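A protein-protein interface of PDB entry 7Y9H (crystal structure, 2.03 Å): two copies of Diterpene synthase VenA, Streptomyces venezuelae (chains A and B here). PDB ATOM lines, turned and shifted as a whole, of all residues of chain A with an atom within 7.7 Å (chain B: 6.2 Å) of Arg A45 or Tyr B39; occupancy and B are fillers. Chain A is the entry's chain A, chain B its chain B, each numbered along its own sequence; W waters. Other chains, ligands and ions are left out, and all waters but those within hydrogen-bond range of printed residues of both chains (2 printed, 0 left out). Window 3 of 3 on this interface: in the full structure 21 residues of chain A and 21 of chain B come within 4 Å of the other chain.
The backbone carbonyl oxygen (O) of Trp B343 sits at hydrogen-bond distance from the side-chain amide nitrogen (ND2) of Asn A51, 3.5 Å away.
The backbone carbonyl oxygen (O) of Glu A47 lies close to the side-chain amide oxygen (OD1) of Asn A51 (3.3 Å).
OH of Tyr B39 is in hydrogen-bond range of OE2 of Glu B328 (2.4 Å).
OD1 of Asp A42 lies within salt-bridge range of NH2 of Arg A45 (3.3 Å).
Pro A41 touches Pro B41.
Ala A44 touches Tyr B39 (CB to CD2, 3.8 Å).
Ala A44 touches Ile B78.
Arg A45 touches Tyr B39.
Leu B332 touches Ile A48 (CD2 to CD1, 3.8 Å).
Ile A48 touches Trp B343.
Tyr B39 touches just these residues of chain A: Ala A44 (3.8 Å) and Arg A45 (3.96 Å).
No residue of chain A comes within 4 Å of Gly B38.
Printed residues of chain B within 4 Å of Asn A51: Trp B343.
Of the printed residues of chain B, Ile A48 touches Leu B332 and Trp B343.
Of the printed residues of chain A, Ile B78 touches Ala A44 (3.6 Å).
The nearest residue of chain B that does not touch Arg A45 is Glu B328 (5.2 Å).
The nearest printed residue of chain A that does not touch Leu B332 is Ala A44 (6.5 Å).
Of the 15 printed residues of chain B, 5 touch a printed residue of chain A.
Printed residues of chain B that touch a printed residue of chain A: Tyr B39, Pro B41, Ile B78, Leu B332 and Trp B343.
Hydrophobic or aromatic side chains of chain B that line the printed part of chain A: Tyr B39, Ile B78, Leu B332 and Trp B343.
Of the 18 printed residues of chain A, 5 touch a printed residue of chain B.
Printed residues of chain A that touch a printed residue of chain B: Pro A41, Ala A44, Arg A45, Ile A48 and Asn A51.
Hydrophobic or aromatic side chains of chain A within 4 Å of the printed part of chain B: Ala A44 and Ile A48.
Among the printed residues, 7 pairs touch across the chains.
Pro A41 touches its own counterpart, Pro B41.
6 positions are printed for both chains.
Water W1 lies within hydrogen-bond range of O of His B40 (2.6 Å) and O of Pro A41 (2.6 Å).
Water W2 lies within hydrogen-bond range of the backbone carbonyl oxygen of Pro A41 (2.7 Å) and the backbone carbonyl oxygen of Tyr B39 (2.8 Å).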
ATOM      1  N   HIS A  40      -0.668  11.736   5.449  1.00  0.00           N
ATOM      2  CA  HIS A  40      -1.271  11.435   4.138  1.00  0.00           C
ATOM      3  C   HIS A  40      -0.219  11.753   3.089  1.00  0.00           C
ATOM      4  O   HIS A  40       0.535  12.713   3.240  1.00  0.00           O
ATOM      5  CB  HIS A  40      -2.561  12.249   3.977  1.00  0.00           C
ATOM      6  CG  HIS A  40      -3.364  11.804   2.822  1.00  0.00           C
ATOM      7  ND1 HIS A  40      -2.999  12.093   1.545  1.00  0.00           N
ATOM      8  CD2 HIS A  40      -4.445  11.007   2.749  1.00  0.00           C
ATOM      9  CE1 HIS A  40      -3.852  11.536   0.713  1.00  0.00           C
ATOM     10  NE2 HIS A  40      -4.740  10.855   1.423  1.00  0.00           N
ATOM     11  N   PRO A  41      -0.090  10.961   2.012  1.00  0.00           N
ATOM     12  CA  PRO A  41       0.926  11.262   0.993  1.00  0.00           C
ATOM     13  C   PRO A  41       0.719  12.626   0.305  1.00  0.00           C
ATOM     14  O   PRO A  41       1.677  13.132  -0.219  1.00  0.00           O
ATOM     15  CB  PRO A  41       0.837  10.097  -0.004  1.00  0.00           C
ATOM     16  CG  PRO A  41      -0.504   9.448   0.290  1.00  0.00           C
ATOM     17  CD  PRO A  41      -0.767   9.682   1.769  1.00  0.00           C
ATOM     18  N   ASP A  42      -0.474  13.223   0.403  1.00  0.00           N
ATOM     19  CA  ASP A  42      -0.755  14.589  -0.106  1.00  0.00           C
ATOM     20  C   ASP A  42      -0.947  15.612   1.029  1.00  0.00           C
ATOM     21  O   ASP A  42      -1.569  16.652   0.782  1.00  0.00           O
ATOM     22  CB  ASP A  42      -2.018  14.578  -0.954  1.00  0.00           C
ATOM     23  CG  ASP A  42      -1.954  13.584  -2.076  1.00  0.00           C
ATOM     24  OD1 ASP A  42      -0.941  13.625  -2.817  1.00  0.00           O
ATOM     25  OD2 ASP A  42      -2.867  12.723  -2.120  1.00  0.00           O
ATOM     26  N   ALA A  43      -0.384  15.380   2.204  1.00  0.00           N
ATOM     27  CA  ALA A  43      -0.699  16.177   3.414  1.00  0.00           C
ATOM     28  C   ALA A  43      -0.394  17.650   3.152  1.00  0.00           C
ATOM     29  O   ALA A  43      -1.270  18.462   3.488  1.00  0.00           O
ATOM     30  CB  ALA A  43       0.072  15.670   4.601  1.00  0.00           C
ATOM     31  N   ALA A  44       0.805  17.984   2.643  1.00  0.00           N
ATOM     32  CA  ALA A  44       1.219  19.400   2.468  1.00  0.00           C
ATOM     33  C   ALA A  44       0.194  20.125   1.581  1.00  0.00           C
ATOM     34  O   ALA A  44      -0.272  21.215   1.941  1.00  0.00           O
ATOM     35  CB  ALA A  44       2.602  19.475   1.889  1.00  0.00           C
ATOM     36  N   ARG A  45      -0.171  19.489   0.475  1.00  0.00           N
ATOM     37  CA  ARG A  45      -1.101  20.023  -0.531  1.00  0.00           C
ATOM     38  C   ARG A  45      -2.510  20.094   0.061  1.00  0.00           C
ATOM     39  O   ARG A  45      -3.215  21.095  -0.213  1.00  0.00           O
ATOM     40  CB  ARG A  45      -1.019  19.201  -1.820  1.00  0.00           C
ATOM     41  CG  ARG A  45      -1.817  19.835  -2.947  1.00  0.00           C
ATOM     42  CD  ARG A  45      -1.577  19.202  -4.316  1.00  0.00           C
ATOM     43  NE  ARG A  45      -1.805  17.783  -4.251  1.00  0.00           N
ATOM     44  CZ  ARG A  45      -2.994  17.196  -4.096  1.00  0.00           C
ATOM     45  NH1 ARG A  45      -4.112  17.907  -4.015  1.00  0.00           N
ATOM     46  NH2 ARG A  45      -3.056  15.875  -4.010  1.00  0.00           N
ATOM     47  N   ILE A  46      -2.921  19.116   0.866  1.00  0.00           N
ATOM     48  CA  ILE A  46      -4.298  19.144   1.434  1.00  0.00           C
ATOM     49  C   ILE A  46      -4.399  20.340   2.405  1.00  0.00           C
ATOM     50  O   ILE A  46      -5.440  21.000   2.470  1.00  0.00           O
ATOM     51  CB  ILE A  46      -4.641  17.792   2.075  1.00  0.00           C
ATOM     52  CG1 ILE A  46      -4.886  16.730   1.006  1.00  0.00           C
ATOM     53  CG2 ILE A  46      -5.850  17.933   2.996  1.00  0.00           C
ATOM     54  CD1 ILE A  46      -4.899  15.300   1.518  1.00  0.00           C
ATOM     55  N   GLU A  47      -3.338  20.645   3.118  1.00  0.00           N
ATOM     56  CA  GLU A  47      -3.319  21.770   4.086  1.00  0.00           C
ATOM     57  C   GLU A  47      -3.565  23.073   3.329  1.00  0.00           C
ATOM     58  O   GLU A  47      -4.457  23.867   3.771  1.00  0.00           O
ATOM     59  CB  GLU A  47      -1.987  21.793   4.836  1.00  0.00           C
ATOM     60  CG  GLU A  47      -1.856  22.978   5.778  1.00  0.00           C
ATOM     61  CD  GLU A  47      -0.491  23.085   6.441  1.00  0.00           C
ATOM     62  OE1 GLU A  47       0.426  22.330   6.011  1.00  0.00           O
ATOM     63  OE2 GLU A  47      -0.324  23.921   7.376  1.00  0.00           O
ATOM     64  N   ILE A  48      -2.797  23.294   2.250  1.00  0.00           N
ATOM     65  CA  ILE A  48      -2.930  24.521   1.413  1.00  0.00           C
ATOM     66  C   ILE A  48      -4.361  24.630   0.881  1.00  0.00           C
ATOM     67  O   ILE A  48      -4.943  25.720   0.935  1.00  0.00           O
ATOM     68  CB  ILE A  48      -1.896  24.509   0.258  1.00  0.00           C
ATOM     69  CG1 ILE A  48      -0.461  24.464   0.766  1.00  0.00           C
ATOM     70  CG2 ILE A  48      -2.144  25.688  -0.671  1.00  0.00           C
ATOM     71  CD1 ILE A  48      -0.237  25.347   1.976  1.00  0.00           C
ATOM     72  N   ALA A  49      -4.864  23.571   0.246  1.00  0.00           N
ATOM     73  CA  ALA A  49      -6.233  23.558  -0.298  1.00  0.00           C
ATOM     74  C   ALA A  49      -7.238  23.816   0.835  1.00  0.00           C
ATOM     75  O   ALA A  49      -8.319  24.436   0.576  1.00  0.00           O
ATOM     76  CB  ALA A  49      -6.489  22.260  -1.025  1.00  0.00           C
ATOM     77  N   SER A  50      -6.954  23.336   2.050  1.00  0.00           N
ATOM     78  CA  SER A  50      -7.892  23.480   3.196  1.00  0.00           C
ATOM     79  C   SER A  50      -7.867  24.955   3.635  1.00  0.00           C
ATOM     80  O   SER A  50      -8.947  25.535   3.891  1.00  0.00           O
ATOM     81  CB  SER A  50      -7.592  22.540   4.332  1.00  0.00           C
ATOM     82  OG  SER A  50      -8.529  22.715   5.396  1.00  0.00           O
ATOM     83  N   ASN A  51      -6.695  25.572   3.586  1.00  0.00           N
ATOM     84  CA  ASN A  51      -6.532  27.030   3.808  1.00  0.00           C
ATOM     85  C   ASN A  51      -7.347  27.780   2.751  1.00  0.00           C
ATOM     86  O   ASN A  51      -8.024  28.736   3.111  1.00  0.00           O
ATOM     87  CB  ASN A  51      -5.063  27.454   3.763  1.00  0.00           C
ATOM     88  CG  ASN A  51      -4.244  26.828   4.864  1.00  0.00           C
ATOM     89  OD1 ASN A  51      -4.788  26.404   5.872  1.00  0.00           O
ATOM     90  ND2 ASN A  51      -2.938  26.818   4.703  1.00  0.00           N
ATOM     91  N   GLY A  52      -7.295  27.347   1.493  1.00  0.00           N
ATOM     92  CA  GLY A  52      -8.144  27.924   0.434  1.00  0.00           C
ATOM     93  C   GLY A  52      -9.628  27.801   0.772  1.00  0.00           C
ATOM     94  O   GLY A  52     -10.337  28.782   0.577  1.00  0.00           O
ATOM     95  N   GLY A  77      -5.139  22.872   8.985  1.00  0.00           N
ATOM     96  CA  GLY A  77      -5.339  22.142   7.730  1.00  0.00           C
ATOM     97  C   GLY A  77      -4.525  20.861   7.611  1.00  0.00           C
ATOM     98  O   GLY A  77      -4.879  20.044   6.738  1.00  0.00           O
ATOM     99  N   ILE A  78      -3.450  20.692   8.388  1.00  0.00           N
ATOM    100  CA  ILE A  78      -2.663  19.434   8.391  1.00  0.00           C
ATOM    101  C   ILE A  78      -3.230  18.421   9.407  1.00  0.00           C
ATOM    102  O   ILE A  78      -2.789  17.249   9.338  1.00  0.00           O
ATOM    103  CB  ILE A  78      -1.162  19.693   8.585  1.00  0.00           C
ATOM    104  CG1 ILE A  78      -0.380  18.541   7.960  1.00  0.00           C
ATOM    105  CG2 ILE A  78      -0.762  19.926  10.043  1.00  0.00           C
ATOM    106  CD1 ILE A  78       0.571  18.929   6.897  1.00  0.00           C
ATOM    107  N   PRO A  81      -4.966  15.379   7.259  1.00  0.00           N
ATOM    108  CA  PRO A  81      -3.981  14.466   6.691  1.00  0.00           C
ATOM    109  C   PRO A  81      -3.106  13.709   7.695  1.00  0.00           C
ATOM    110  O   PRO A  81      -2.570  12.639   7.326  1.00  0.00           O
ATOM    111  CB  PRO A  81      -3.053  15.373   5.877  1.00  0.00           C
ATOM    112  CG  PRO A  81      -3.776  16.677   5.707  1.00  0.00           C
ATOM    113  CD  PRO A  81      -4.841  16.746   6.772  1.00  0.00           C
ATOM    114  N   ALA A  89      -7.620  10.895  -1.071  1.00  0.00           N
ATOM    115  CA  ALA A  89      -7.311  12.338  -1.011  1.00  0.00           C
ATOM    116  C   ALA A  89      -8.592  13.141  -0.813  1.00  0.00           C
ATOM    117  O   ALA A  89      -8.540  14.078  -0.026  1.00  0.00           O
ATOM    118  CB  ALA A  89      -6.544  12.777  -2.251  1.00  0.00           C
ATOM    119  N   GLN A  93      -9.302  15.467   2.392  1.00  0.00           N
ATOM    120  CA  GLN A  93      -9.585  16.913   2.204  1.00  0.00           C
ATOM    121  C   GLN A  93     -10.861  17.284   2.972  1.00  0.00           C
ATOM    122  O   GLN A  93     -10.886  18.288   3.671  1.00  0.00           O
ATOM    123  CB  GLN A  93      -9.758  17.284   0.739  1.00  0.00           C
ATOM    124  CG  GLN A  93      -9.868  18.796   0.553  1.00  0.00           C
ATOM    125  CD  GLN A  93      -8.531  19.449   0.849  1.00  0.00           C
ATOM    126  OE1 GLN A  93      -7.527  19.113   0.215  1.00  0.00           O
ATOM    127  NE2 GLN A  93      -8.509  20.370   1.817  1.00  0.00           N
ATOM    128  N   ALA B  37       4.604  19.320 -11.116  1.00  0.00           N
ATOM    129  CA  ALA B  37       4.894  19.910  -9.791  1.00  0.00           C
ATOM    130  C   ALA B  37       4.340  18.943  -8.750  1.00  0.00           C
ATOM    131  O   ALA B  37       3.162  19.000  -8.468  1.00  0.00           O
ATOM    132  CB  ALA B  37       4.280  21.279  -9.658  1.00  0.00           C
ATOM    133  N   GLY B  38       5.153  18.026  -8.272  1.00  0.00           N
ATOM    134  CA  GLY B  38       4.697  17.031  -7.304  1.00  0.00           C
ATOM    135  C   GLY B  38       5.345  17.269  -5.968  1.00  0.00           C
ATOM    136  O   GLY B  38       6.473  17.768  -5.943  1.00  0.00           O
ATOM    137  N   TYR B  39       4.647  16.858  -4.910  1.00  0.00           N
ATOM    138  CA  TYR B  39       5.157  16.832  -3.521  1.00  0.00           C
ATOM    139  C   TYR B  39       5.636  15.414  -3.243  1.00  0.00           C
ATOM    140  O   TYR B  39       4.839  14.505  -3.459  1.00  0.00           O
ATOM    141  CB  TYR B  39       4.064  17.228  -2.528  1.00  0.00           C
ATOM    142  CG  TYR B  39       3.584  18.659  -2.596  1.00  0.00           C
ATOM    143  CD1 TYR B  39       2.734  19.093  -3.605  1.00  0.00           C
ATOM    144  CD2 TYR B  39       3.942  19.564  -1.619  1.00  0.00           C
ATOM    145  CE1 TYR B  39       2.279  20.411  -3.647  1.00  0.00           C
ATOM    146  CE2 TYR B  39       3.474  20.870  -1.640  1.00  0.00           C
ATOM    147  CZ  TYR B  39       2.658  21.300  -2.665  1.00  0.00           C
ATOM    148  OH  TYR B  39       2.229  22.589  -2.669  1.00  0.00           O
ATOM    149  N   HIS B  40       6.871  15.257  -2.772  1.00  0.00           N
ATOM    150  CA  HIS B  40       7.335  14.015  -2.118  1.00  0.00           C
ATOM    151  C   HIS B  40       6.242  13.513  -1.171  1.00  0.00           C
ATOM    152  O   HIS B  40       5.606  14.298  -0.460  1.00  0.00           O
ATOM    153  CB  HIS B  40       8.643  14.233  -1.360  1.00  0.00           C
ATOM    154  CG  HIS B  40       9.323  12.946  -1.058  1.00  0.00           C
ATOM    155  ND1 HIS B  40       8.890  12.117  -0.055  1.00  0.00           N
ATOM    156  CD2 HIS B  40      10.316  12.283  -1.691  1.00  0.00           C
ATOM    157  CE1 HIS B  40       9.617  11.016  -0.045  1.00  0.00           C
ATOM    158  NE2 HIS B  40      10.510  11.095  -1.016  1.00  0.00           N
ATOM    159  N   PRO B  41       5.951  12.192  -1.163  1.00  0.00           N
ATOM    160  CA  PRO B  41       4.977  11.635  -0.234  1.00  0.00           C
ATOM    161  C   PRO B  41       5.257  11.970   1.232  1.00  0.00           C
ATOM    162  O   PRO B  41       4.317  11.904   1.973  1.00  0.00           O
ATOM    163  CB  PRO B  41       5.086  10.102  -0.426  1.00  0.00           C
ATOM    164  CG  PRO B  41       5.654   9.946  -1.828  1.00  0.00           C
ATOM    165  CD  PRO B  41       6.514  11.176  -2.072  1.00  0.00           C
ATOM    166  N   ASP B  42       6.510  12.245   1.601  1.00  0.00           N
ATOM    167  CA  ASP B  42       6.907  12.625   2.979  1.00  0.00           C
ATOM    168  C   ASP B  42       7.217  14.118   3.132  1.00  0.00           C
ATOM    169  O   ASP B  42       7.881  14.443   4.124  1.00  0.00           O
ATOM    170  CB  ASP B  42       8.112  11.819   3.436  1.00  0.00           C
ATOM    171  CG  ASP B  42       7.868  10.321   3.358  1.00  0.00           C
ATOM    172  OD1 ASP B  42       6.842   9.862   3.902  1.00  0.00           O
ATOM    173  OD2 ASP B  42       8.709   9.640   2.762  1.00  0.00           O
ATOM    174  N   ALA B  43       6.700  14.980   2.256  1.00  0.00           N
ATOM    175  CA  ALA B  43       7.065  16.412   2.186  1.00  0.00           C
ATOM    176  C   ALA B  43       6.834  17.100   3.542  1.00  0.00           C
ATOM    177  O   ALA B  43       7.767  17.746   4.063  1.00  0.00           O
ATOM    178  CB  ALA B  43       6.290  17.099   1.075  1.00  0.00           C
ATOM    179  N   ILE B  78      10.475  22.725   2.765  1.00  0.00           N
ATOM    180  CA  ILE B  78       9.596  21.958   1.832  1.00  0.00           C
ATOM    181  C   ILE B  78      10.052  22.146   0.358  1.00  0.00           C
ATOM    182  O   ILE B  78       9.498  21.473  -0.496  1.00  0.00           O
ATOM    183  CB  ILE B  78       8.104  22.273   2.019  1.00  0.00           C
ATOM    184  CG1 ILE B  78       7.267  21.051   1.627  1.00  0.00           C
ATOM    185  CG2 ILE B  78       7.687  23.519   1.229  1.00  0.00           C
ATOM    186  CD1 ILE B  78       5.822  21.162   1.992  1.00  0.00           C
ATOM    187  N   PRO B  81      11.552  18.485  -0.984  1.00  0.00           N
ATOM    188  CA  PRO B  81      10.502  17.549  -1.335  1.00  0.00           C
ATOM    189  C   PRO B  81       9.648  17.966  -2.527  1.00  0.00           C
ATOM    190  O   PRO B  81       9.103  17.111  -3.164  1.00  0.00           O
ATOM    191  CB  PRO B  81       9.602  17.466  -0.093  1.00  0.00           C
ATOM    192  CG  PRO B  81      10.401  18.078   1.026  1.00  0.00           C
ATOM    193  CD  PRO B  81      11.510  18.903   0.419  1.00  0.00           C
ATOM    194  N   LEU B  82       9.543  19.270  -2.792  1.00  0.00           N
ATOM    195  CA  LEU B  82       8.828  19.775  -3.986  1.00  0.00           C
ATOM    196  C   LEU B  82       9.719  19.628  -5.232  1.00  0.00           C
ATOM    197  O   LEU B  82       9.170  19.591  -6.332  1.00  0.00           O
ATOM    198  CB  LEU B  82       8.361  21.220  -3.766  1.00  0.00           C
ATOM    199  CG  LEU B  82       6.919  21.361  -3.282  1.00  0.00           C
ATOM    200  CD1 LEU B  82       6.647  22.802  -2.854  1.00  0.00           C
ATOM    201  CD2 LEU B  82       5.917  20.943  -4.339  1.00  0.00           C
ATOM    202  N   PRO B  85      10.302  14.961  -5.762  1.00  0.00           N
ATOM    203  CA  PRO B  85       9.199  14.202  -5.163  1.00  0.00           C
ATOM    204  C   PRO B  85       9.294  12.686  -5.433  1.00  0.00           C
ATOM    205  O   PRO B  85       8.675  11.920  -4.726  1.00  0.00           O
ATOM    206  CB  PRO B  85       7.971  14.781  -5.869  1.00  0.00           C
ATOM    207  CG  PRO B  85       8.516  15.150  -7.227  1.00  0.00           C
ATOM    208  CD  PRO B  85       9.847  15.788  -6.895  1.00  0.00           C
ATOM    209  N   GLU B 328       5.934  25.911  -7.751  1.00  0.00           N
ATOM    210  CA  GLU B 328       4.947  25.586  -6.694  1.00  0.00           C
ATOM    211  C   GLU B 328       5.527  26.134  -5.386  1.00  0.00           C
ATOM    212  O   GLU B 328       4.838  26.873  -4.672  1.00  0.00           O
ATOM    213  CB  GLU B 328       4.711  24.078  -6.619  1.00  0.00           C
ATOM    214  CG  GLU B 328       3.770  23.645  -5.489  1.00  0.00           C
ATOM    215  CD  GLU B 328       2.284  23.748  -5.767  1.00  0.00           C
ATOM    216  OE1 GLU B 328       1.902  24.265  -6.824  1.00  0.00           O
ATOM    217  OE2 GLU B 328       1.503  23.359  -4.875  1.00  0.00           O
ATOM    218  N   PHE B 329       6.792  25.842  -5.113  1.00  0.00           N
ATOM    219  CA  PHE B 329       7.444  26.298  -3.873  1.00  0.00           C
ATOM    220  C   PHE B 329       7.393  27.834  -3.771  1.00  0.00           C
ATOM    221  O   PHE B 329       7.206  28.416  -2.647  1.00  0.00           O
ATOM    222  CB  PHE B 329       8.889  25.814  -3.757  1.00  0.00           C
ATOM    223  CG  PHE B 329       9.552  26.452  -2.576  1.00  0.00           C
ATOM    224  CD1 PHE B 329       9.209  26.044  -1.290  1.00  0.00           C
ATOM    225  CD2 PHE B 329      10.474  27.470  -2.736  1.00  0.00           C
ATOM    226  CE1 PHE B 329       9.766  26.662  -0.182  1.00  0.00           C
ATOM    227  CE2 PHE B 329      11.019  28.101  -1.625  1.00  0.00           C
ATOM    228  CZ  PHE B 329      10.674  27.692  -0.357  1.00  0.00           C
ATOM    229  N   LEU B 332       4.382  29.355  -2.514  1.00  0.00           N
ATOM    230  CA  LEU B 332       4.060  28.809  -1.158  1.00  0.00           C
ATOM    231  C   LEU B 332       4.767  29.653  -0.071  1.00  0.00           C
ATOM    232  O   LEU B 332       4.208  29.866   1.048  1.00  0.00           O
ATOM    233  CB  LEU B 332       4.487  27.329  -1.199  1.00  0.00           C
ATOM    234  CG  LEU B 332       4.451  26.472   0.067  1.00  0.00           C
ATOM    235  CD1 LEU B 332       5.617  26.793   0.999  1.00  0.00           C
ATOM    236  CD2 LEU B 332       3.148  26.622   0.795  1.00  0.00           C
ATOM    237  N   TRP B 343      -0.018  30.381   2.385  1.00  0.00           N
ATOM    238  CA  TRP B 343      -0.527  30.182   1.006  1.00  0.00           C
ATOM    239  C   TRP B 343      -1.932  29.555   1.047  1.00  0.00           C
ATOM    240  O   TRP B 343      -2.154  28.611   1.852  1.00  0.00           O
ATOM    241  CB  TRP B 343       0.464  29.332   0.212  1.00  0.00           C
ATOM    242  CG  TRP B 343       0.190  29.303  -1.253  1.00  0.00           C
ATOM    243  CD1 TRP B 343      -0.356  30.303  -2.007  1.00  0.00           C
ATOM    244  CD2 TRP B 343       0.446  28.207  -2.149  1.00  0.00           C
ATOM    245  NE1 TRP B 343      -0.454  29.904  -3.302  1.00  0.00           N
ATOM    246  CE2 TRP B 343       0.059  28.639  -3.429  1.00  0.00           C
ATOM    247  CE3 TRP B 343       1.039  26.950  -2.007  1.00  0.00           C
ATOM    248  CZ2 TRP B 343       0.155  27.818  -4.543  1.00  0.00           C
ATOM    249  CZ3 TRP B 343       1.177  26.147  -3.117  1.00  0.00           C
ATOM    250  CH2 TRP B 343       0.743  26.585  -4.372  1.00  0.00           C
HETATM  251  O   HOH W   1       3.229  15.258   0.074  1.00  0.00           O
HETATM  252  O   HOH W   2       2.689  12.896  -2.742  1.00  0.00           O
